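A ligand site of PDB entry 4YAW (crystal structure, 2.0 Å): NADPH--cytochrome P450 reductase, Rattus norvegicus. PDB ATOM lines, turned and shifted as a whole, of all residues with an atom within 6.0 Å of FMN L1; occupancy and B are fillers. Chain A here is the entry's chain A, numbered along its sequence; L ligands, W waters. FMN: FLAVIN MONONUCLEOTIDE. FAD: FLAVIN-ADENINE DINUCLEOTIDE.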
ATOM      1  N   GLY A  29      -0.583  37.900 -18.719  1.00  0.00           N
ATOM      2  CA  GLY A  29       0.499  37.885 -17.759  1.00  0.00           C
ATOM      3  C   GLY A  29       1.370  36.729 -18.182  1.00  0.00           C
ATOM      4  O   GLY A  29       1.017  35.568 -18.005  1.00  0.00           O
ATOM      5  N   SER A  30       2.520  37.062 -18.762  1.00  0.00           N
ATOM      6  CA  SER A  30       3.387  36.048 -19.336  1.00  0.00           C
ATOM      7  C   SER A  30       4.842  36.343 -19.041  1.00  0.00           C
ATOM      8  O   SER A  30       5.244  37.492 -18.899  1.00  0.00           O
ATOM      9  CB  SER A  30       3.173  35.977 -20.853  1.00  0.00           C
ATOM     10  OG  SER A  30       3.967  34.962 -21.437  1.00  0.00           O
ATOM     11  N   GLN A  31       5.647  35.283 -18.964  1.00  0.00           N
ATOM     12  CA  GLN A  31       7.069  35.454 -18.719  1.00  0.00           C
ATOM     13  C   GLN A  31       7.878  34.702 -19.766  1.00  0.00           C
ATOM     14  O   GLN A  31       9.006  35.073 -20.071  1.00  0.00           O
ATOM     15  CB  GLN A  31       7.420  34.958 -17.315  1.00  0.00           C
ATOM     16  CG  GLN A  31       8.649  35.613 -16.722  1.00  0.00           C
ATOM     17  CD  GLN A  31       8.538  35.813 -15.221  1.00  0.00           C
ATOM     18  OE1 GLN A  31       7.656  36.531 -14.745  1.00  0.00           O
ATOM     19  NE2 GLN A  31       9.435  35.189 -14.480  1.00  0.00           N
ATOM     20  N   THR A  32       7.280  33.660 -20.344  1.00  0.00           N
ATOM     21  CA  THR A  32       7.930  32.862 -21.378  1.00  0.00           C
ATOM     22  C   THR A  32       7.129  32.955 -22.673  1.00  0.00           C
ATOM     23  O   THR A  32       7.286  32.141 -23.575  1.00  0.00           O
ATOM     24  CB  THR A  32       8.058  31.381 -20.937  1.00  0.00           C
ATOM     25  OG1 THR A  32       8.812  31.300 -19.728  1.00  0.00           O
ATOM     26  CG2 THR A  32       8.765  30.564 -22.005  1.00  0.00           C
ATOM     27  N   GLY A  33       6.245  33.950 -22.752  1.00  0.00           N
ATOM     28  CA  GLY A  33       5.457  34.164 -23.947  1.00  0.00           C
ATOM     29  C   GLY A  33       4.258  33.267 -24.215  1.00  0.00           C
ATOM     30  O   GLY A  33       3.504  33.517 -25.156  1.00  0.00           O
ATOM     31  N   THR A  34       4.067  32.233 -23.402  1.00  0.00           N
ATOM     32  CA  THR A  34       2.949  31.323 -23.621  1.00  0.00           C
ATOM     33  C   THR A  34       1.595  32.040 -23.499  1.00  0.00           C
ATOM     34  O   THR A  34       0.752  31.944 -24.404  1.00  0.00           O
ATOM     35  CB  THR A  34       2.969  30.149 -22.635  1.00  0.00           C
ATOM     36  OG1 THR A  34       4.277  29.541 -22.644  1.00  0.00           O
ATOM     37  CG2 THR A  34       1.937  29.099 -23.028  1.00  0.00           C
ATOM     38  N   ALA A  35       1.390  32.737 -22.393  1.00  0.00           N
ATOM     39  CA  ALA A  35       0.128  33.446 -22.161  1.00  0.00           C
ATOM     40  C   ALA A  35      -0.083  34.537 -23.211  1.00  0.00           C
ATOM     41  O   ALA A  35      -1.219  34.865 -23.549  1.00  0.00           O
ATOM     42  CB  ALA A  35       0.123  34.067 -20.754  1.00  0.00           C
ATOM     43  N   GLU A  36       1.021  35.083 -23.712  1.00  0.00           N
ATOM     44  CA  GLU A  36       0.920  36.113 -24.732  1.00  0.00           C
ATOM     45  C   GLU A  36       0.339  35.491 -25.998  1.00  0.00           C
ATOM     46  O   GLU A  36      -0.528  36.083 -26.641  1.00  0.00           O
ATOM     47  CB  GLU A  36       2.291  36.721 -25.038  1.00  0.00           C
ATOM     48  CG  GLU A  36       2.204  38.024 -25.805  1.00  0.00           C
ATOM     49  CD  GLU A  36       3.551  38.669 -26.069  1.00  0.00           C
ATOM     50  OE1 GLU A  36       4.369  38.776 -25.131  1.00  0.00           O
ATOM     51  OE2 GLU A  36       3.789  39.082 -27.222  1.00  0.00           O
ATOM     52  N   ALA A  82      -0.267  33.573 -16.230  1.00  0.00           N
ATOM     53  CA  ALA A  82       0.588  32.481 -15.782  1.00  0.00           C
ATOM     54  C   ALA A  82       1.008  32.815 -14.350  1.00  0.00           C
ATOM     55  O   ALA A  82       0.932  33.972 -13.924  1.00  0.00           O
ATOM     56  CB  ALA A  82       1.823  32.372 -16.676  1.00  0.00           C
ATOM     57  N   THR A  83       1.443  31.803 -13.615  1.00  0.00           N
ATOM     58  CA  THR A  83       1.909  32.008 -12.243  1.00  0.00           C
ATOM     59  C   THR A  83       3.394  31.653 -12.172  1.00  0.00           C
ATOM     60  O   THR A  83       3.844  30.715 -12.834  1.00  0.00           O
ATOM     61  CB  THR A  83       1.155  31.115 -11.245  1.00  0.00           C
ATOM     62  OG1 THR A  83      -0.228  31.485 -11.207  1.00  0.00           O
ATOM     63  CG2 THR A  83       1.751  31.246  -9.851  1.00  0.00           C
ATOM     64  N   TYR A  84       4.145  32.411 -11.381  1.00  0.00           N
ATOM     65  CA  TYR A  84       5.579  32.174 -11.222  1.00  0.00           C
ATOM     66  C   TYR A  84       6.011  32.320  -9.774  1.00  0.00           C
ATOM     67  O   TYR A  84       5.850  33.379  -9.168  1.00  0.00           O
ATOM     68  CB  TYR A  84       6.371  33.143 -12.104  1.00  0.00           C
ATOM     69  CG  TYR A  84       6.581  32.651 -13.524  1.00  0.00           C
ATOM     70  CD1 TYR A  84       5.610  32.864 -14.491  1.00  0.00           C
ATOM     71  CD2 TYR A  84       7.736  31.973 -13.886  1.00  0.00           C
ATOM     72  CE1 TYR A  84       5.789  32.418 -15.793  1.00  0.00           C
ATOM     73  CE2 TYR A  84       7.926  31.531 -15.181  1.00  0.00           C
ATOM     74  CZ  TYR A  84       6.948  31.751 -16.127  1.00  0.00           C
ATOM     75  OH  TYR A  84       7.128  31.310 -17.421  1.00  0.00           O
ATOM     76  N   GLU A  85       6.452  31.135  -9.217  1.00  0.00           N
ATOM     77  CA  GLU A  85       6.863  31.080  -7.820  1.00  0.00           C
ATOM     78  C   GLU A  85       5.725  31.533  -6.918  1.00  0.00           C
ATOM     79  O   GLU A  85       5.947  32.164  -5.885  1.00  0.00           O
ATOM     80  CB  GLU A  85       8.083  31.981  -7.602  1.00  0.00           C
ATOM     81  CG  GLU A  85       9.307  31.567  -8.414  1.00  0.00           C
ATOM     82  CD  GLU A  85      10.466  32.530  -8.235  1.00  0.00           C
ATOM     83  OE1 GLU A  85      10.343  33.697  -8.670  1.00  0.00           O
ATOM     84  OE2 GLU A  85      11.504  32.123  -7.669  1.00  0.00           O
ATOM     85  N   GLY A  86       4.488  31.202  -7.310  1.00  0.00           N
ATOM     86  CA  GLY A  86       3.334  31.583  -6.517  1.00  0.00           C
ATOM     87  C   GLY A  86       2.968  33.056  -6.650  1.00  0.00           C
ATOM     88  O   GLY A  86       2.062  33.538  -5.976  1.00  0.00           O
ATOM     89  N   ASP A  87       3.660  33.775  -7.527  1.00  0.00           N
ATOM     90  CA  ASP A  87       3.378  35.192  -7.715  1.00  0.00           C
ATOM     91  C   ASP A  87       2.968  35.526  -9.148  1.00  0.00           C
ATOM     92  O   ASP A  87       2.939  34.646 -10.023  1.00  0.00           O
ATOM     93  CB  ASP A  87       4.605  36.040  -7.363  1.00  0.00           C
ATOM     94  CG  ASP A  87       4.918  36.022  -5.879  1.00  0.00           C
ATOM     95  OD1 ASP A  87       4.031  36.399  -5.072  1.00  0.00           O
ATOM     96  OD2 ASP A  87       6.049  35.648  -5.519  1.00  0.00           O
ATOM     97  N   THR A  89       3.341  37.218 -12.909  1.00  0.00           N
ATOM     98  CA  THR A  89       4.502  37.311 -13.771  1.00  0.00           C
ATOM     99  C   THR A  89       4.968  38.756 -13.595  1.00  0.00           C
ATOM    100  O   THR A  89       4.200  39.604 -13.129  1.00  0.00           O
ATOM    101  CB  THR A  89       4.132  37.040 -15.250  1.00  0.00           C
ATOM    102  OG1 THR A  89       3.062  37.907 -15.651  1.00  0.00           O
ATOM    103  CG2 THR A  89       3.715  35.597 -15.435  1.00  0.00           C
ATOM    104  N   LEU A 116      -2.544  29.973 -16.444  1.00  0.00           N
ATOM    105  CA  LEU A 116      -1.470  29.109 -16.909  1.00  0.00           C
ATOM    106  C   LEU A 116      -0.649  28.738 -15.681  1.00  0.00           C
ATOM    107  O   LEU A 116      -0.094  29.603 -14.995  1.00  0.00           O
ATOM    108  CB  LEU A 116      -0.570  29.825 -17.928  1.00  0.00           C
ATOM    109  CG  LEU A 116      -1.125  30.147 -19.321  1.00  0.00           C
ATOM    110  CD1 LEU A 116      -2.006  31.386 -19.266  1.00  0.00           C
ATOM    111  CD2 LEU A 116       0.044  30.380 -20.269  1.00  0.00           C
ATOM    112  N   GLY A 117      -0.581  27.440 -15.411  1.00  0.00           N
ATOM    113  CA  GLY A 117       0.161  26.962 -14.256  1.00  0.00           C
ATOM    114  C   GLY A 117       0.755  25.579 -14.466  1.00  0.00           C
ATOM    115  O   GLY A 117       0.875  25.099 -15.600  1.00  0.00           O
ATOM    116  N   ASN A 118       1.108  24.943 -13.365  1.00  0.00           N
ATOM    117  CA  ASN A 118       1.713  23.617 -13.392  1.00  0.00           C
ATOM    118  C   ASN A 118       1.432  22.957 -12.034  1.00  0.00           C
ATOM    119  O   ASN A 118       1.885  23.445 -10.996  1.00  0.00           O
ATOM    120  CB  ASN A 118       3.223  23.763 -13.615  1.00  0.00           C
ATOM    121  CG  ASN A 118       3.925  22.447 -13.773  1.00  0.00           C
ATOM    122  OD1 ASN A 118       3.760  21.527 -12.959  1.00  0.00           O
ATOM    123  ND2 ASN A 118       4.724  22.337 -14.829  1.00  0.00           N
ATOM    124  N   LYS A 119       0.675  21.861 -12.052  1.00  0.00           N
ATOM    125  CA  LYS A 119       0.301  21.169 -10.819  1.00  0.00           C
ATOM    126  C   LYS A 119       1.446  20.742  -9.895  1.00  0.00           C
ATOM    127  O   LYS A 119       1.217  20.533  -8.702  1.00  0.00           O
ATOM    128  CB  LYS A 119      -0.565  19.946 -11.128  1.00  0.00           C
ATOM    129  CG  LYS A 119      -2.020  20.256 -11.494  1.00  0.00           C
ATOM    130  CD  LYS A 119      -2.810  18.963 -11.629  1.00  0.00           C
ATOM    131  CE  LYS A 119      -4.295  19.227 -11.837  1.00  0.00           C
ATOM    132  NZ  LYS A 119      -4.548  20.000 -13.082  1.00  0.00           N
ATOM    133  N   TYR A 121       3.730  22.465  -8.723  1.00  0.00           N
ATOM    134  CA  TYR A 121       4.126  23.530  -7.801  1.00  0.00           C
ATOM    135  C   TYR A 121       3.149  23.705  -6.646  1.00  0.00           C
ATOM    136  O   TYR A 121       1.971  23.401  -6.761  1.00  0.00           O
ATOM    137  CB  TYR A 121       4.296  24.854  -8.542  1.00  0.00           C
ATOM    138  CG  TYR A 121       5.500  24.885  -9.461  1.00  0.00           C
ATOM    139  CD1 TYR A 121       5.434  24.322 -10.737  1.00  0.00           C
ATOM    140  CD2 TYR A 121       6.697  25.465  -9.062  1.00  0.00           C
ATOM    141  CE1 TYR A 121       6.538  24.345 -11.592  1.00  0.00           C
ATOM    142  CE2 TYR A 121       7.815  25.488  -9.897  1.00  0.00           C
ATOM    143  CZ  TYR A 121       7.720  24.924 -11.168  1.00  0.00           C
ATOM    144  OH  TYR A 121       8.805  24.950 -12.010  1.00  0.00           O
ATOM    145  N   GLU A 122       3.666  24.212  -5.529  1.00  0.00           N
ATOM    146  CA  GLU A 122       2.892  24.426  -4.314  1.00  0.00           C
ATOM    147  C   GLU A 122       1.601  25.201  -4.560  1.00  0.00           C
ATOM    148  O   GLU A 122       0.515  24.745  -4.212  1.00  0.00           O
ATOM    149  CB  GLU A 122       3.748  25.175  -3.293  1.00  0.00           C
ATOM    150  CG  GLU A 122       3.097  25.296  -1.923  1.00  0.00           C
ATOM    151  CD  GLU A 122       2.913  23.957  -1.262  1.00  0.00           C
ATOM    152  OE1 GLU A 122       3.940  23.307  -0.929  1.00  0.00           O
ATOM    153  OE2 GLU A 122       1.745  23.530  -1.080  1.00  0.00           O
ATOM    154  N   HIS A 123       1.746  26.395  -5.138  1.00  0.00           N
ATOM    155  CA  HIS A 123       0.617  27.263  -5.419  1.00  0.00           C
ATOM    156  C   HIS A 123       0.246  27.220  -6.901  1.00  0.00           C
ATOM    157  O   HIS A 123       0.653  28.071  -7.690  1.00  0.00           O
ATOM    158  CB  HIS A 123       0.974  28.686  -5.006  1.00  0.00           C
ATOM    159  CG  HIS A 123       1.520  28.776  -3.618  1.00  0.00           C
ATOM    160  ND1 HIS A 123       0.736  28.588  -2.498  1.00  0.00           N
ATOM    161  CD2 HIS A 123       2.774  28.984  -3.162  1.00  0.00           C
ATOM    162  CE1 HIS A 123       1.491  28.675  -1.409  1.00  0.00           C
ATOM    163  NE2 HIS A 123       2.735  28.910  -1.783  1.00  0.00           N
ATOM    164  N   PHE A 124      -0.537  26.204  -7.261  1.00  0.00           N
ATOM    165  CA  PHE A 124      -0.972  25.982  -8.630  1.00  0.00           C
ATOM    166  C   PHE A 124      -1.960  27.012  -9.161  1.00  0.00           C
ATOM    167  O   PHE A 124      -3.070  27.159  -8.625  1.00  0.00           O
ATOM    168  CB  PHE A 124      -1.576  24.577  -8.723  1.00  0.00           C
ATOM    169  CG  PHE A 124      -2.210  24.278 -10.037  1.00  0.00           C
ATOM    170  CD1 PHE A 124      -1.473  24.347 -11.217  1.00  0.00           C
ATOM    171  CD2 PHE A 124      -3.550  23.930 -10.106  1.00  0.00           C
ATOM    172  CE1 PHE A 124      -2.072  24.067 -12.445  1.00  0.00           C
ATOM    173  CE2 PHE A 124      -4.159  23.649 -11.332  1.00  0.00           C
ATOM    174  CZ  PHE A 124      -3.408  23.718 -12.492  1.00  0.00           C
ATOM    175  N   ASN A 125      -1.566  27.713 -10.224  1.00  0.00           N
ATOM    176  CA  ASN A 125      -2.418  28.721 -10.846  1.00  0.00           C
ATOM    177  C   ASN A 125      -2.877  29.793  -9.866  1.00  0.00           C
ATOM    178  O   ASN A 125      -3.978  30.325  -9.968  1.00  0.00           O
ATOM    179  CB  ASN A 125      -3.628  28.061 -11.505  1.00  0.00           C
ATOM    180  CG  ASN A 125      -3.419  27.796 -12.982  1.00  0.00           C
ATOM    181  OD1 ASN A 125      -3.071  28.694 -13.750  1.00  0.00           O
ATOM    182  ND2 ASN A 125      -3.620  26.548 -13.389  1.00  0.00           N
ATOM    183  N   ALA A 126      -2.002  30.093  -8.902  1.00  0.00           N
ATOM    184  CA  ALA A 126      -2.286  31.088  -7.872  1.00  0.00           C
ATOM    185  C   ALA A 126      -2.696  32.446  -8.444  1.00  0.00           C
ATOM    186  O   ALA A 126      -3.584  33.088  -7.911  1.00  0.00           O
ATOM    187  CB  ALA A 126      -1.069  31.251  -6.969  1.00  0.00           C
ATOM    188  N   ASP A 151       0.541  22.917 -17.185  1.00  0.00           N
ATOM    189  CA  ASP A 151       1.681  22.605 -18.040  1.00  0.00           C
ATOM    190  C   ASP A 151       2.365  21.288 -17.685  1.00  0.00           C
ATOM    191  O   ASP A 151       3.319  20.879 -18.355  1.00  0.00           O
ATOM    192  CB  ASP A 151       2.693  23.764 -18.002  1.00  0.00           C
ATOM    193  CG  ASP A 151       3.647  23.747 -19.191  1.00  0.00           C
ATOM    194  OD1 ASP A 151       3.225  23.373 -20.306  1.00  0.00           O
ATOM    195  OD2 ASP A 151       4.824  24.114 -19.004  1.00  0.00           O
ATOM    196  N   LEU A 155      -0.836  21.754 -21.490  1.00  0.00           N
ATOM    197  CA  LEU A 155      -1.446  23.069 -21.435  1.00  0.00           C
ATOM    198  C   LEU A 155      -2.230  23.389 -22.690  1.00  0.00           C
ATOM    199  O   LEU A 155      -3.349  23.893 -22.622  1.00  0.00           O
ATOM    200  CB  LEU A 155      -0.371  24.138 -21.191  1.00  0.00           C
ATOM    201  CG  LEU A 155      -0.776  25.606 -21.094  1.00  0.00           C
ATOM    202  CD1 LEU A 155      -1.823  25.795 -19.988  1.00  0.00           C
ATOM    203  CD2 LEU A 155       0.455  26.439 -20.780  1.00  0.00           C
ATOM    204  N   VAL A 619      13.792  24.750  -8.228  1.00  0.00           N
ATOM    205  CA  VAL A 619      13.544  23.551  -8.992  1.00  0.00           C
ATOM    206  C   VAL A 619      12.973  23.845 -10.369  1.00  0.00           C
ATOM    207  O   VAL A 619      12.317  24.852 -10.590  1.00  0.00           O
ATOM    208  CB  VAL A 619      12.589  22.605  -8.214  1.00  0.00           C
ATOM    209  CG1 VAL A 619      13.272  22.128  -6.939  1.00  0.00           C
ATOM    210  CG2 VAL A 619      11.297  23.338  -7.866  1.00  0.00           C
HETATM  211  N1  FMN L   1       2.875  27.328 -12.183  1.00  0.00           N
HETATM  212  C2  FMN L   1       2.061  27.423 -11.107  1.00  0.00           C
HETATM  213  O2  FMN L   1       0.879  27.122 -11.190  1.00  0.00           O
HETATM  214  N3  FMN L   1       2.631  27.872  -9.939  1.00  0.00           N
HETATM  215  C4  FMN L   1       3.965  28.234  -9.731  1.00  0.00           C
HETATM  216  O4  FMN L   1       4.239  28.602  -8.589  1.00  0.00           O
HETATM  217  C4A FMN L   1       4.834  28.139 -10.849  1.00  0.00           C
HETATM  218  N5  FMN L   1       6.196  28.485 -10.661  1.00  0.00           N
HETATM  219  C5A FMN L   1       6.978  28.344 -11.810  1.00  0.00           C
HETATM  220  C6  FMN L   1       8.365  28.680 -11.655  1.00  0.00           C
HETATM  221  C7  FMN L   1       9.281  28.584 -12.736  1.00  0.00           C
HETATM  222  C7M FMN L   1      10.738  28.980 -12.408  1.00  0.00           C
HETATM  223  C8  FMN L   1       8.811  28.127 -14.082  1.00  0.00           C
HETATM  224  C8M FMN L   1       9.598  27.984 -15.210  1.00  0.00           C
HETATM  225  C9  FMN L   1       7.473  27.793 -14.247  1.00  0.00           C
HETATM  226  C9A FMN L   1       6.521  27.895 -13.141  1.00  0.00           C
HETATM  227  N10 FMN L   1       5.084  27.558 -13.232  1.00  0.00           N
HETATM  228  C10 FMN L   1       4.218  27.673 -12.046  1.00  0.00           C
HETATM  229  C1' FMN L   1       4.538  27.107 -14.492  1.00  0.00           C
HETATM  230  C2' FMN L   1       4.088  28.255 -15.441  1.00  0.00           C
HETATM  231  O2' FMN L   1       3.055  29.082 -14.767  1.00  0.00           O
HETATM  232  C3' FMN L   1       3.545  27.653 -16.722  1.00  0.00           C
HETATM  233  O3' FMN L   1       4.621  26.899 -17.313  1.00  0.00           O
HETATM  234  C4' FMN L   1       3.058  28.817 -17.649  1.00  0.00           C
HETATM  235  O4' FMN L   1       2.557  28.061 -18.791  1.00  0.00           O
HETATM  236  C5' FMN L   1       4.151  29.723 -18.176  1.00  0.00           C
HETATM  237  O5' FMN L   1       3.584  30.811 -19.001  1.00  0.00           O
HETATM  238  P   FMN L   1       4.362  31.942 -19.755  1.00  0.00           P
HETATM  239  O1P FMN L   1       5.165  31.333 -20.854  1.00  0.00           O
HETATM  240  O2P FMN L   1       5.082  32.743 -18.624  1.00  0.00           O
HETATM  241  O3P FMN L   1       3.138  32.751 -20.403  1.00  0.00           O
HETATM  242  PA  FAD L   2      15.452  23.103 -25.123  1.00  0.00           P
HETATM  243  O1A FAD L   2      15.636  23.271 -26.579  1.00  0.00           O
HETATM  244  O2A FAD L   2      14.844  24.194 -24.338  1.00  0.00           O
HETATM  245  O5B FAD L   2      14.635  21.733 -24.866  1.00  0.00           O
HETATM  246  C5B FAD L   2      14.103  21.432 -23.571  1.00  0.00           C
HETATM  247  C4B FAD L   2      12.958  20.433 -23.735  1.00  0.00           C
HETATM  248  O4B FAD L   2      13.397  19.249 -24.407  1.00  0.00           O
HETATM  249  C3B FAD L   2      12.474  19.915 -22.396  1.00  0.00           C
HETATM  250  O3B FAD L   2      11.624  20.901 -21.789  1.00  0.00           O
HETATM  251  C2B FAD L   2      11.629  18.762 -22.906  1.00  0.00           C
HETATM  252  O2B FAD L   2      10.381  19.249 -23.429  1.00  0.00           O
HETATM  253  C1B FAD L   2      12.484  18.210 -24.039  1.00  0.00           C
HETATM  254  N9A FAD L   2      13.312  17.062 -23.584  1.00  0.00           N
HETATM  255  C8A FAD L   2      14.584  17.142 -22.841  1.00  0.00           C
HETATM  256  N7A FAD L   2      14.930  15.715 -22.748  1.00  0.00           N
HETATM  257  C5A FAD L   2      13.972  15.000 -23.324  1.00  0.00           C
HETATM  258  C6A FAD L   2      13.882  13.679 -23.473  1.00  0.00           C
HETATM  259  N6A FAD L   2      14.874  12.959 -22.959  1.00  0.00           N
HETATM  260  N1A FAD L   2      12.812  13.084 -24.018  1.00  0.00           N
HETATM  261  C2A FAD L   2      11.741  13.886 -24.445  1.00  0.00           C
HETATM  262  N3A FAD L   2      11.855  15.260 -24.258  1.00  0.00           N
HETATM  263  C4A FAD L   2      12.970  15.784 -23.710  1.00  0.00           C
HETATM  264  N1  FAD L   2      19.332  23.629 -16.314  1.00  0.00           N
HETATM  265  C2  FAD L   2      20.648  23.294 -15.991  1.00  0.00           C
HETATM  266  O2  FAD L   2      21.195  22.359 -16.571  1.00  0.00           O
HETATM  267  N3  FAD L   2      21.313  23.987 -14.969  1.00  0.00           N
HETATM  268  C4  FAD L   2      20.653  25.004 -14.264  1.00  0.00           C
HETATM  269  O4  FAD L   2      21.295  25.705 -13.475  1.00  0.00           O
HETATM  270  C4X FAD L   2      19.340  25.312 -14.575  1.00  0.00           C
HETATM  271  N5  FAD L   2      18.642  26.162 -13.789  1.00  0.00           N
HETATM  272  C5X FAD L   2      17.370  26.462 -14.103  1.00  0.00           C
HETATM  273  C6  FAD L   2      16.676  27.385 -13.328  1.00  0.00           C
HETATM  274  C7  FAD L   2      15.376  27.735 -13.671  1.00  0.00           C
HETATM  275  C7M FAD L   2      14.750  28.787 -12.998  1.00  0.00           C
HETATM  276  C8  FAD L   2      14.763  27.156 -14.774  1.00  0.00           C
HETATM  277  C8M FAD L   2      13.461  27.501 -15.126  1.00  0.00           C
HETATM  278  C9  FAD L   2      15.465  26.242 -15.555  1.00  0.00           C
HETATM  279  C9A FAD L   2      16.780  25.917 -15.236  1.00  0.00           C
HETATM  280  N10 FAD L   2      17.489  25.080 -16.019  1.00  0.00           N
HETATM  281  C10 FAD L   2      18.676  24.632 -15.592  1.00  0.00           C
HETATM  282  C1' FAD L   2      16.902  24.505 -17.250  1.00  0.00           C
HETATM  283  C2' FAD L   2      17.276  25.404 -18.432  1.00  0.00           C
HETATM  284  O2' FAD L   2      16.634  26.677 -18.287  1.00  0.00           O
HETATM  285  C3' FAD L   2      16.901  24.799 -19.794  1.00  0.00           C
HETATM  286  O3' FAD L   2      15.522  24.415 -19.808  1.00  0.00           O
HETATM  287  C4' FAD L   2      17.795  23.597 -20.101  1.00  0.00           C
HETATM  288  O4' FAD L   2      19.171  23.987 -20.046  1.00  0.00           O
HETATM  289  C5' FAD L   2      17.471  23.058 -21.502  1.00  0.00           C
HETATM  290  O5' FAD L   2      17.494  24.137 -22.441  1.00  0.00           O
HETATM  291  P   FAD L   2      17.894  23.914 -23.979  1.00  0.00           P
HETATM  292  O1P FAD L   2      19.260  23.365 -24.045  1.00  0.00           O
HETATM  293  O2P FAD L   2      17.592  25.163 -24.709  1.00  0.00           O
HETATM  294  O3P FAD L   2      16.882  22.753 -24.459  1.00  0.00           O
HETATM  295  O   HOH W   1       4.225  27.541  -6.043  1.00  0.00           O
HETATM  296  O   HOH W   2       7.560  27.412 -18.143  1.00  0.00           O
HETATM  297  O   HOH W   3      11.127  30.422 -16.813  1.00  0.00           O
HETATM  298  O   HOH W   4       4.427  27.256 -21.117  1.00  0.00           O
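Water W1 lies within hydrogen-bond range of an oxygen (O4) of FMN L1 (2.8 Å), the backbone NH (N) of His 123 (2.9 Å) and the backbone NH (N) of Glu 122 (3.4 Å).
Water W4 bridges OG1 of Thr 34 and O4' of FMN L1.
OG of Ser 30 is in hydrogen-bond range of N of Thr 34, 3.4 Å away.
The side-chain hydroxyl of Ser 30 sits at hydrogen-bond distance from the backbone NH of Gly 33 (2.8 Å).
The side-chain hydroxyl (OG1) of Thr 89 is in hydrogen-bond range of the backbone NH (N) of Ser 30 (3.3 Å).
The backbone carbonyl oxygen of Leu 116 is in hydrogen-bond range of the backbone NH of Thr 83.
N of Ala 126 sits at hydrogen-bond distance from OG1 of Thr 83 (3.2 Å).
The side-chain amide oxygen (OD1) of Asn 125 sits at hydrogen-bond distance from the backbone NH (N) of Leu 116, at 3.0 Å.
OH of Tyr 84 lies within hydrogen-bond range of OG1 of Thr 32.
The backbone NH (N) of Asp 151 sits at hydrogen-bond distance from the backbone carbonyl oxygen (O) of Gly 117 (2.7 Å).
Ala 82 touches FMN L1 (CB to O5', 3.3 Å).
CA of Gly 117 touches O2 of FMN L1, 3.2 Å away.
Tyr 121 touches FMN L1.
CA of Phe 124 touches O2 of FMN L1, 3.4 Å away.
Leu 155 touches FMN L1 (CD2 to O4', 3.3 Å).
Hydrophobic or aromatic side chains that line FMN L1: Ala 35, Ala 82, Tyr 84, Leu 116, Tyr 121, Phe 124 and Leu 155.
Of the 28 residues printed, 20 come within 4 Å of FMN L1.
The side-chain hydroxyl of Ser 30 sits at hydrogen-bond distance from an oxygen (O3P) of FMN L1, at 2.6 Å.
N of Gln 31 sits at hydrogen-bond distance from O2P of FMN L1 (2.6 Å).
N of Ala 35 sits at hydrogen-bond distance from O3P of FMN L1, at 2.6 Å.
An oxygen (O2') of FMN L1 sits at hydrogen-bond distance from the backbone NH (N) of Thr 83.
O of Thr 83 is in hydrogen-bond range of O2' of FMN L1, 2.7 Å away.
N of Thr 34 sits at hydrogen-bond distance from O1P of FMN L1 (2.9 Å).
An oxygen (O1P) of FMN L1 lies within hydrogen-bond range of the side-chain hydroxyl (OG1) of Thr 34, 2.7 Å away.
The backbone NH (N) of Asn 125 is in hydrogen-bond range of an oxygen (O2) of FMN L1, at 2.7 Å.
OH of Tyr 84 lies within hydrogen-bond range of O2P of FMN L1, at 2.8 Å.
N of Thr 32 is in hydrogen-bond range of O2P of FMN L1 (2.9 Å).
The backbone NH (N) of Gly 86 sits at hydrogen-bond distance from an oxygen (O4) of FMN L1 (2.9 Å).
A nitrogen (N3) of FMN L1 sits at hydrogen-bond distance from the backbone carbonyl oxygen (O) of His 123 (3.0 Å).
The backbone NH of Glu 85 lies within hydrogen-bond range of a nitrogen (N5) of FMN L1 (3.0 Å).
N of Asn 118 sits at hydrogen-bond distance from O2 of FMN L1, at 3.1 Å.
An oxygen (O2') of FMN L1 sits at hydrogen-bond distance from the backbone carbonyl oxygen of Leu 116 (3.2 Å).
The side-chain carboxylate (OD2) of Asp 151 sits at hydrogen-bond distance from an oxygen (O3') of FMN L1 (3.3 Å).
An oxygen (O1P) of FMN L1 is in hydrogen-bond range of the backbone NH of Gly 33, at 3.4 Å.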
